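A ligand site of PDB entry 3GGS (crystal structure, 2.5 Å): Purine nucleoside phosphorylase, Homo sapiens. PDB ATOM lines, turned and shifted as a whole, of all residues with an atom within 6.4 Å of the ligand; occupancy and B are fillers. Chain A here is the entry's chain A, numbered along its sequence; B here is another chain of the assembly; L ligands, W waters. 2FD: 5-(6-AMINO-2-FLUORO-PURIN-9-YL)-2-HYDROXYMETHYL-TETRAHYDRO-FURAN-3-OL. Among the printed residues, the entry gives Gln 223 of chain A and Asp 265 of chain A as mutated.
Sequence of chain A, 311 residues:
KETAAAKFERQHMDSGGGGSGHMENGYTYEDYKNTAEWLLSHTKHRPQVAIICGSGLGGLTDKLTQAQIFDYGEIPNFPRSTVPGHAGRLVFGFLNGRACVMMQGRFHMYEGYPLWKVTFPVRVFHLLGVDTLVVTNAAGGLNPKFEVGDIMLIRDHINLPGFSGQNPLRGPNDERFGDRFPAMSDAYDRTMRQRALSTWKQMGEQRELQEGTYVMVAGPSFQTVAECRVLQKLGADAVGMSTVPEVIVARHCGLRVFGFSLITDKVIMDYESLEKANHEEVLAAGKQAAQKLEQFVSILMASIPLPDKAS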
ATOM      1  N   GLY A  54      -5.485  14.731  11.176  1.00  0.00           N
ATOM      2  CA  GLY A  54      -5.840  14.188  12.461  1.00  0.00           C
ATOM      3  C   GLY A  54      -5.951  15.246  13.534  1.00  0.00           C
ATOM      4  O   GLY A  54      -5.782  16.450  13.280  1.00  0.00           O
ATOM      5  N   SER A  55      -6.226  14.805  14.747  1.00  0.00           N
ATOM      6  CA  SER A  55      -6.426  15.689  15.879  1.00  0.00           C
ATOM      7  C   SER A  55      -5.128  16.440  16.231  1.00  0.00           C
ATOM      8  O   SER A  55      -4.088  15.821  16.436  1.00  0.00           O
ATOM      9  CB  SER A  55      -6.945  14.900  17.074  1.00  0.00           C
ATOM     10  OG  SER A  55      -7.424  15.756  18.086  1.00  0.00           O
ATOM     11  N   HIS A 108     -15.666  10.491  13.679  1.00  0.00           N
ATOM     12  CA  HIS A 108     -15.175   9.311  14.402  1.00  0.00           C
ATOM     13  C   HIS A 108     -16.338   8.386  14.766  1.00  0.00           C
ATOM     14  O   HIS A 108     -17.489   8.818  14.939  1.00  0.00           O
ATOM     15  CB  HIS A 108     -14.439   9.677  15.687  1.00  0.00           C
ATOM     16  CG  HIS A 108     -13.281  10.594  15.496  1.00  0.00           C
ATOM     17  ND1 HIS A 108     -13.417  11.967  15.432  1.00  0.00           N
ATOM     18  CD2 HIS A 108     -11.951  10.350  15.407  1.00  0.00           C
ATOM     19  CE1 HIS A 108     -12.231  12.516  15.285  1.00  0.00           C
ATOM     20  NE2 HIS A 108     -11.317  11.559  15.259  1.00  0.00           N
ATOM     21  N   TYR A 110     -16.583   6.635  17.591  1.00  0.00           N
ATOM     22  CA  TYR A 110     -16.954   6.912  18.986  1.00  0.00           C
ATOM     23  C   TYR A 110     -17.943   8.044  19.183  1.00  0.00           C
ATOM     24  O   TYR A 110     -18.579   8.103  20.225  1.00  0.00           O
ATOM     25  CB  TYR A 110     -15.733   7.141  19.872  1.00  0.00           C
ATOM     26  CG  TYR A 110     -14.867   8.336  19.543  1.00  0.00           C
ATOM     27  CD1 TYR A 110     -13.542   8.155  19.134  1.00  0.00           C
ATOM     28  CD2 TYR A 110     -15.346   9.642  19.678  1.00  0.00           C
ATOM     29  CE1 TYR A 110     -12.743   9.244  18.834  1.00  0.00           C
ATOM     30  CE2 TYR A 110     -14.538  10.728  19.381  1.00  0.00           C
ATOM     31  CZ  TYR A 110     -13.237  10.518  18.948  1.00  0.00           C
ATOM     32  OH  TYR A 110     -12.432  11.587  18.642  1.00  0.00           O
ATOM     33  N   ASN A 137      -2.897  10.998  11.854  1.00  0.00           N
ATOM     34  CA  ASN A 137      -3.646  10.857  13.101  1.00  0.00           C
ATOM     35  C   ASN A 137      -2.705  11.004  14.281  1.00  0.00           C
ATOM     36  O   ASN A 137      -1.485  10.986  14.119  1.00  0.00           O
ATOM     37  CB  ASN A 137      -4.370   9.492  13.162  1.00  0.00           C
ATOM     38  CG  ASN A 137      -3.413   8.297  13.232  1.00  0.00           C
ATOM     39  OD1 ASN A 137      -2.446   8.291  14.014  1.00  0.00           O
ATOM     40  ND2 ASN A 137      -3.681   7.284  12.414  1.00  0.00           N
ATOM     41  N   ALA A 138      -3.292  11.179  15.458  1.00  0.00           N
ATOM     42  CA  ALA A 138      -2.566  11.135  16.726  1.00  0.00           C
ATOM     43  C   ALA A 138      -2.776   9.736  17.304  1.00  0.00           C
ATOM     44  O   ALA A 138      -3.820   9.128  17.100  1.00  0.00           O
ATOM     45  CB  ALA A 138      -3.092  12.195  17.685  1.00  0.00           C
ATOM     46  N   ALA A 139      -1.781   9.234  18.027  1.00  0.00           N
ATOM     47  CA  ALA A 139      -1.847   7.875  18.548  1.00  0.00           C
ATOM     48  C   ALA A 139      -1.064   7.688  19.830  1.00  0.00           C
ATOM     49  O   ALA A 139      -0.073   8.383  20.082  1.00  0.00           O
ATOM     50  CB  ALA A 139      -1.375   6.886  17.488  1.00  0.00           C
ATOM     51  N   GLY A 140      -1.532   6.744  20.649  1.00  0.00           N
ATOM     52  CA  GLY A 140      -0.785   6.282  21.794  1.00  0.00           C
ATOM     53  C   GLY A 140       0.247   5.290  21.310  1.00  0.00           C
ATOM     54  O   GLY A 140      -0.046   4.442  20.468  1.00  0.00           O
ATOM     55  N   GLY A 141       1.466   5.393  21.842  1.00  0.00           N
ATOM     56  CA  GLY A 141       2.515   4.473  21.481  1.00  0.00           C
ATOM     57  C   GLY A 141       2.380   3.194  22.289  1.00  0.00           C
ATOM     58  O   GLY A 141       2.292   3.252  23.511  1.00  0.00           O
ATOM     59  N   LEU A 142       2.355   2.050  21.603  1.00  0.00           N
ATOM     60  CA  LEU A 142       2.460   0.749  22.267  1.00  0.00           C
ATOM     61  C   LEU A 142       3.938   0.213  22.301  1.00  0.00           C
ATOM     62  O   LEU A 142       4.275  -0.647  23.113  1.00  0.00           O
ATOM     63  CB  LEU A 142       1.505  -0.242  21.606  1.00  0.00           C
ATOM     64  CG  LEU A 142       0.018   0.205  21.505  1.00  0.00           C
ATOM     65  CD1 LEU A 142      -0.742  -0.612  20.466  1.00  0.00           C
ATOM     66  CD2 LEU A 142      -0.731   0.169  22.858  1.00  0.00           C
ATOM     67  N   VAL A 215      -3.099   0.065  15.263  1.00  0.00           N
ATOM     68  CA  VAL A 215      -4.276  -0.697  15.667  1.00  0.00           C
ATOM     69  C   VAL A 215      -5.438   0.264  15.944  1.00  0.00           C
ATOM     70  O   VAL A 215      -5.276   1.262  16.669  1.00  0.00           O
ATOM     71  CB  VAL A 215      -3.965  -1.639  16.871  1.00  0.00           C
ATOM     72  CG1 VAL A 215      -3.767  -0.867  18.158  1.00  0.00           C
ATOM     73  CG2 VAL A 215      -5.046  -2.689  17.030  1.00  0.00           C
ATOM     74  N   VAL A 217      -8.936   0.874  17.702  1.00  0.00           N
ATOM     75  CA  VAL A 217      -9.946   0.483  18.680  1.00  0.00           C
ATOM     76  C   VAL A 217     -11.100   1.486  18.540  1.00  0.00           C
ATOM     77  O   VAL A 217     -10.876   2.612  18.111  1.00  0.00           O
ATOM     78  CB  VAL A 217      -9.358   0.494  20.085  1.00  0.00           C
ATOM     79  CG1 VAL A 217      -8.156  -0.495  20.160  1.00  0.00           C
ATOM     80  CG2 VAL A 217      -8.922   1.921  20.485  1.00  0.00           C
ATOM     81  N   GLY A 219     -12.793   3.056  20.768  1.00  0.00           N
ATOM     82  CA  GLY A 219     -12.893   4.015  21.874  1.00  0.00           C
ATOM     83  C   GLY A 219     -14.353   4.265  22.260  1.00  0.00           C
ATOM     84  O   GLY A 219     -15.242   3.513  21.842  1.00  0.00           O
ATOM     85  N   PRO A 220     -14.628   5.354  22.994  1.00  0.00           N
ATOM     86  CA  PRO A 220     -13.773   6.490  23.337  1.00  0.00           C
ATOM     87  C   PRO A 220     -12.989   6.346  24.626  1.00  0.00           C
ATOM     88  O   PRO A 220     -12.040   7.102  24.836  1.00  0.00           O
ATOM     89  CB  PRO A 220     -14.772   7.632  23.473  1.00  0.00           C
ATOM     90  CG  PRO A 220     -15.970   6.971  24.042  1.00  0.00           C
ATOM     91  CD  PRO A 220     -16.025   5.605  23.423  1.00  0.00           C
ATOM     92  N   SER A 221     -13.396   5.427  25.485  1.00  0.00           N
ATOM     93  CA  SER A 221     -12.634   5.108  26.699  1.00  0.00           C
ATOM     94  C   SER A 221     -11.210   4.744  26.305  1.00  0.00           C
ATOM     95  O   SER A 221     -10.977   4.249  25.202  1.00  0.00           O
ATOM     96  CB  SER A 221     -13.265   3.908  27.448  1.00  0.00           C
ATOM     97  OG  SER A 221     -12.363   2.794  27.467  1.00  0.00           O
ATOM     98  N   PHE A 222     -10.267   4.945  27.201  1.00  0.00           N
ATOM     99  CA  PHE A 222      -8.868   4.528  26.963  1.00  0.00           C
ATOM    100  C   PHE A 222      -8.565   3.145  27.544  1.00  0.00           C
ATOM    101  O   PHE A 222      -9.273   2.650  28.407  1.00  0.00           O
ATOM    102  CB  PHE A 222      -7.902   5.559  27.563  1.00  0.00           C
ATOM    103  CG  PHE A 222      -7.536   6.673  26.626  1.00  0.00           C
ATOM    104  CD1 PHE A 222      -8.311   6.979  25.507  1.00  0.00           C
ATOM    105  CD2 PHE A 222      -6.422   7.445  26.887  1.00  0.00           C
ATOM    106  CE1 PHE A 222      -7.948   8.030  24.649  1.00  0.00           C
ATOM    107  CE2 PHE A 222      -6.068   8.499  26.025  1.00  0.00           C
ATOM    108  CZ  PHE A 222      -6.842   8.780  24.909  1.00  0.00           C
ATOM    109  N   GLN A 223      -7.452   2.574  27.079  1.00  0.00           N
ATOM    110  CA  GLN A 223      -7.035   1.231  27.457  1.00  0.00           C
ATOM    111  C   GLN A 223      -6.783   1.057  28.954  1.00  0.00           C
ATOM    112  O   GLN A 223      -6.406   1.996  29.637  1.00  0.00           O
ATOM    113  CB  GLN A 223      -5.774   0.828  26.683  1.00  0.00           C
ATOM    114  CG  GLN A 223      -6.040   0.308  25.259  1.00  0.00           C
ATOM    115  CD  GLN A 223      -7.206   0.989  24.532  1.00  0.00           C
ATOM    116  OE1 GLN A 223      -8.353   0.520  24.577  1.00  0.00           O
ATOM    117  NE2 GLN A 223      -6.900   2.100  23.839  1.00  0.00           N
ATOM    118  N   VAL A 239      -1.733   2.772  18.889  1.00  0.00           N
ATOM    119  CA  VAL A 239      -3.172   2.648  18.932  1.00  0.00           C
ATOM    120  C   VAL A 239      -3.810   3.997  18.724  1.00  0.00           C
ATOM    121  O   VAL A 239      -3.212   5.024  19.099  1.00  0.00           O
ATOM    122  CB  VAL A 239      -3.685   2.036  20.290  1.00  0.00           C
ATOM    123  CG1 VAL A 239      -3.147   2.794  21.472  1.00  0.00           C
ATOM    124  CG2 VAL A 239      -5.260   2.014  20.313  1.00  0.00           C
ATOM    125  N   GLY A 240      -4.995   3.984  18.116  1.00  0.00           N
ATOM    126  CA  GLY A 240      -5.850   5.163  17.956  1.00  0.00           C
ATOM    127  C   GLY A 240      -7.249   4.739  17.508  1.00  0.00           C
ATOM    128  O   GLY A 240      -7.516   3.551  17.341  1.00  0.00           O
ATOM    129  N   MET A 241      -8.151   5.696  17.265  1.00  0.00           N
ATOM    130  CA  MET A 241      -9.580   5.383  17.053  1.00  0.00           C
ATOM    131  C   MET A 241     -10.117   5.830  15.693  1.00  0.00           C
ATOM    132  O   MET A 241     -11.318   6.142  15.563  1.00  0.00           O
ATOM    133  CB  MET A 241     -10.431   6.033  18.142  1.00  0.00           C
ATOM    134  CG  MET A 241      -9.803   6.013  19.529  1.00  0.00           C
ATOM    135  SD  MET A 241     -10.749   6.959  20.737  1.00  0.00           S
ATOM    136  CE  MET A 241      -9.927   6.414  22.239  1.00  0.00           C
ATOM    137  N   SER A 242      -9.248   5.840  14.684  1.00  0.00           N
ATOM    138  CA  SER A 242      -9.623   6.392  13.375  1.00  0.00           C
ATOM    139  C   SER A 242      -8.834   5.779  12.213  1.00  0.00           C
ATOM    140  O   SER A 242      -8.146   4.786  12.397  1.00  0.00           O
ATOM    141  CB  SER A 242      -9.424   7.918  13.394  1.00  0.00           C
ATOM    142  OG  SER A 242      -8.051   8.263  13.273  1.00  0.00           O
ATOM    143  N   LEU A 262       1.121  10.497  14.737  1.00  0.00           N
ATOM    144  CA  LEU A 262       1.887  11.286  15.696  1.00  0.00           C
ATOM    145  C   LEU A 262       1.711  10.677  17.073  1.00  0.00           C
ATOM    146  O   LEU A 262       0.585  10.611  17.566  1.00  0.00           O
ATOM    147  CB  LEU A 262       1.421  12.742  15.712  1.00  0.00           C
ATOM    148  CG  LEU A 262       2.275  13.675  16.585  1.00  0.00           C
ATOM    149  CD1 LEU A 262       3.683  13.786  16.021  1.00  0.00           C
ATOM    150  CD2 LEU A 262       1.650  15.043  16.689  1.00  0.00           C
ATOM    151  N   THR A 264       1.410  10.876  20.611  1.00  0.00           N
ATOM    152  CA  THR A 264       1.112  11.937  21.584  1.00  0.00           C
ATOM    153  C   THR A 264       1.309  11.537  23.052  1.00  0.00           C
ATOM    154  O   THR A 264       1.492  12.417  23.891  1.00  0.00           O
ATOM    155  CB  THR A 264      -0.325  12.492  21.411  1.00  0.00           C
ATOM    156  OG1 THR A 264      -1.272  11.437  21.560  1.00  0.00           O
ATOM    157  CG2 THR A 264      -0.499  13.136  20.059  1.00  0.00           C
ATOM    158  N   ASP A 265       1.266  10.238  23.361  1.00  0.00           N
ATOM    159  CA  ASP A 265       1.752   9.715  24.664  1.00  0.00           C
ATOM    160  C   ASP A 265       2.111   8.230  24.608  1.00  0.00           C
ATOM    161  O   ASP A 265       1.595   7.501  23.759  1.00  0.00           O
ATOM    162  CB  ASP A 265       0.710   9.938  25.762  1.00  0.00           C
ATOM    163  CG  ASP A 265      -0.487   9.020  25.637  1.00  0.00           C
ATOM    164  OD1 ASP A 265      -1.305   9.230  24.717  1.00  0.00           O
ATOM    165  OD2 ASP A 265      -0.598   8.077  26.448  1.00  0.00           O
ATOM    166  N   VAL A 267       1.464   4.763  26.103  1.00  0.00           N
ATOM    167  CA  VAL A 267       0.462   4.068  26.918  1.00  0.00           C
ATOM    168  C   VAL A 267       1.170   3.234  28.002  1.00  0.00           C
ATOM    169  O   VAL A 267       2.267   2.709  27.763  1.00  0.00           O
ATOM    170  CB  VAL A 267      -0.476   3.172  26.068  1.00  0.00           C
ATOM    171  CG1 VAL A 267      -1.035   3.969  24.896  1.00  0.00           C
ATOM    172  CG2 VAL A 267       0.262   1.962  25.551  1.00  0.00           C
ATOM    173  N   VAL A 282      -2.349  13.214  29.601  1.00  0.00           N
ATOM    174  CA  VAL A 282      -2.213  12.841  28.183  1.00  0.00           C
ATOM    175  C   VAL A 282      -2.608  14.040  27.324  1.00  0.00           C
ATOM    176  O   VAL A 282      -3.774  14.202  26.967  1.00  0.00           O
ATOM    177  CB  VAL A 282      -3.092  11.619  27.792  1.00  0.00           C
ATOM    178  CG1 VAL A 282      -3.044  11.381  26.271  1.00  0.00           C
ATOM    179  CG2 VAL A 282      -2.652  10.361  28.551  1.00  0.00           C
ATOM    180  N   LEU A 283      -1.631  14.907  27.025  1.00  0.00           N
ATOM    181  CA  LEU A 283      -1.922  16.143  26.326  1.00  0.00           C
ATOM    182  C   LEU A 283      -2.075  15.857  24.831  1.00  0.00           C
ATOM    183  O   LEU A 283      -1.780  14.748  24.349  1.00  0.00           O
ATOM    184  CB  LEU A 283      -0.843  17.213  26.593  1.00  0.00           C
ATOM    185  CG  LEU A 283      -1.247  18.707  26.560  1.00  0.00           C
ATOM    186  CD1 LEU A 283      -0.671  19.462  27.758  1.00  0.00           C
ATOM    187  CD2 LEU A 283      -0.854  19.404  25.252  1.00  0.00           C
ATOM    188  N   PHE B 181     -12.728  11.240  26.672  1.00  0.00           N
ATOM    189  CA  PHE B 181     -11.805  10.107  26.610  1.00  0.00           C
ATOM    190  C   PHE B 181     -11.335   9.723  28.002  1.00  0.00           C
ATOM    191  O   PHE B 181     -10.186   9.959  28.344  1.00  0.00           O
ATOM    192  CB  PHE B 181     -10.586  10.463  25.764  1.00  0.00           C
ATOM    193  CG  PHE B 181     -10.918  10.976  24.387  1.00  0.00           C
ATOM    194  CD1 PHE B 181     -11.520  10.137  23.450  1.00  0.00           C
ATOM    195  CD2 PHE B 181     -10.632  12.286  24.022  1.00  0.00           C
ATOM    196  CE1 PHE B 181     -11.828  10.600  22.182  1.00  0.00           C
ATOM    197  CE2 PHE B 181     -10.939  12.750  22.754  1.00  0.00           C
ATOM    198  CZ  PHE B 181     -11.542  11.892  21.832  1.00  0.00           C
HETATM  199  O5' 2FD L   1      -9.416  10.369  19.152  1.00  0.00           O
HETATM  200  C5' 2FD L   1      -8.621  10.014  20.295  1.00  0.00           C
HETATM  201  C4' 2FD L   1      -7.279  10.734  20.250  1.00  0.00           C
HETATM  202  O4' 2FD L   1      -6.498  10.411  21.400  1.00  0.00           O
HETATM  203  C1' 2FD L   1      -5.145  10.106  21.046  1.00  0.00           C
HETATM  204  N9  2FD L   1      -4.626   8.989  21.881  1.00  0.00           N
HETATM  205  C4  2FD L   1      -5.126   7.751  21.997  1.00  0.00           C
HETATM  206  N3  2FD L   1      -6.166   7.091  21.428  1.00  0.00           N
HETATM  207  C2  2FD L   1      -6.435   5.804  21.765  1.00  0.00           C
HETATM  208  F   2FD L   1      -7.476   5.188  21.177  1.00  0.00           F
HETATM  209  N1  2FD L   1      -5.663   5.144  22.668  1.00  0.00           N
HETATM  210  C6  2FD L   1      -4.628   5.781  23.261  1.00  0.00           C
HETATM  211  N6  2FD L   1      -3.819   5.169  24.169  1.00  0.00           N
HETATM  212  C5  2FD L   1      -4.343   7.086  22.929  1.00  0.00           C
HETATM  213  N7  2FD L   1      -3.384   7.942  23.342  1.00  0.00           N
HETATM  214  C8  2FD L   1      -3.575   9.101  22.694  1.00  0.00           C
HETATM  215  C2' 2FD L   1      -5.141   9.782  19.574  1.00  0.00           C
HETATM  216  C3' 2FD L   1      -6.452  10.321  19.038  1.00  0.00           C
HETATM  217  O3' 2FD L   1      -6.220  11.448  18.185  1.00  0.00           O
HETATM  218  O   HOH W   1      -8.896   8.785  17.178  1.00  0.00           O
HETATM  219  O   HOH W   2      -5.659   3.704  25.426  1.00  0.00           O
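The side-chain carboxylate (OD1) of Asp 265 lies within hydrogen-bond range of a nitrogen (N7) of the ligand.
The side-chain hydroxyl (OH) of Tyr 110 lies within hydrogen-bond range of an oxygen (O5') of the ligand.
N of Gly 140 sits close to N7 of the ligand (3.5 Å).
NE2 of Gln 223 lies within hydrogen-bond range of N1 of the ligand (3.5 Å).
O of Asp 265 sits at hydrogen-bond distance from N of Gly 141, 2.9 Å away.
O of Gly 141 sits at hydrogen-bond distance from N of Val 267, 3.1 Å away.
A ring nitrogen (ND1) of His 108 sits at hydrogen-bond distance from the side-chain hydroxyl of Tyr 110 (3.4 Å).
The backbone carbonyl oxygen (O) of Gly 140 sits at hydrogen-bond distance from the backbone NH (N) of Val 239 (2.9 Å).
O of Ala 139 sits at hydrogen-bond distance from N of Thr 264 (2.9 Å).
N of Val 217 lies within hydrogen-bond range of O of Gly 240, 3.1 Å away.
The backbone carbonyl oxygen (O) of Val 215 sits at hydrogen-bond distance from the backbone NH (N) of Gly 240 (3.1 Å).
The backbone carbonyl oxygen (O) of Leu 262 is in hydrogen-bond range of the backbone NH (N) of Ala 139, 2.8 Å away.
The side-chain sulfur (SD) of Met 241 sits close to a fluorine (F) of the ligand.
Merely in contact with the ligand: Ser 55 (3.7 Å), Ala 138 (2.9 Å), Ala 139 (3.7 Å), Val 217 (3.6 Å), Phe 222 (3.5 Å), Val 239 (3.6 Å), Gly 240 (3.6 Å), Thr 264 (3.5 Å), Val 267 (3.1 Å) and Phe 181 of chain B (3.7 Å).
Of the 28 residues printed, 15 come within 4 Å of the ligand.
Along chain A the residues within 4 Å of the ligand span positions 55 to 267.
The nearest printed residue that does not touch the ligand is Val 282 (4.3 Å).
Water W1 bridges O5' of the ligand (2.6 Å) and N of Met 241 (3.2 Å).
Water W2 lies within hydrogen-bond range of the side-chain amide nitrogen (NE2) of Gln 223 (2.6 Å) and a nitrogen (N6) of the ligand (2.7 Å).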
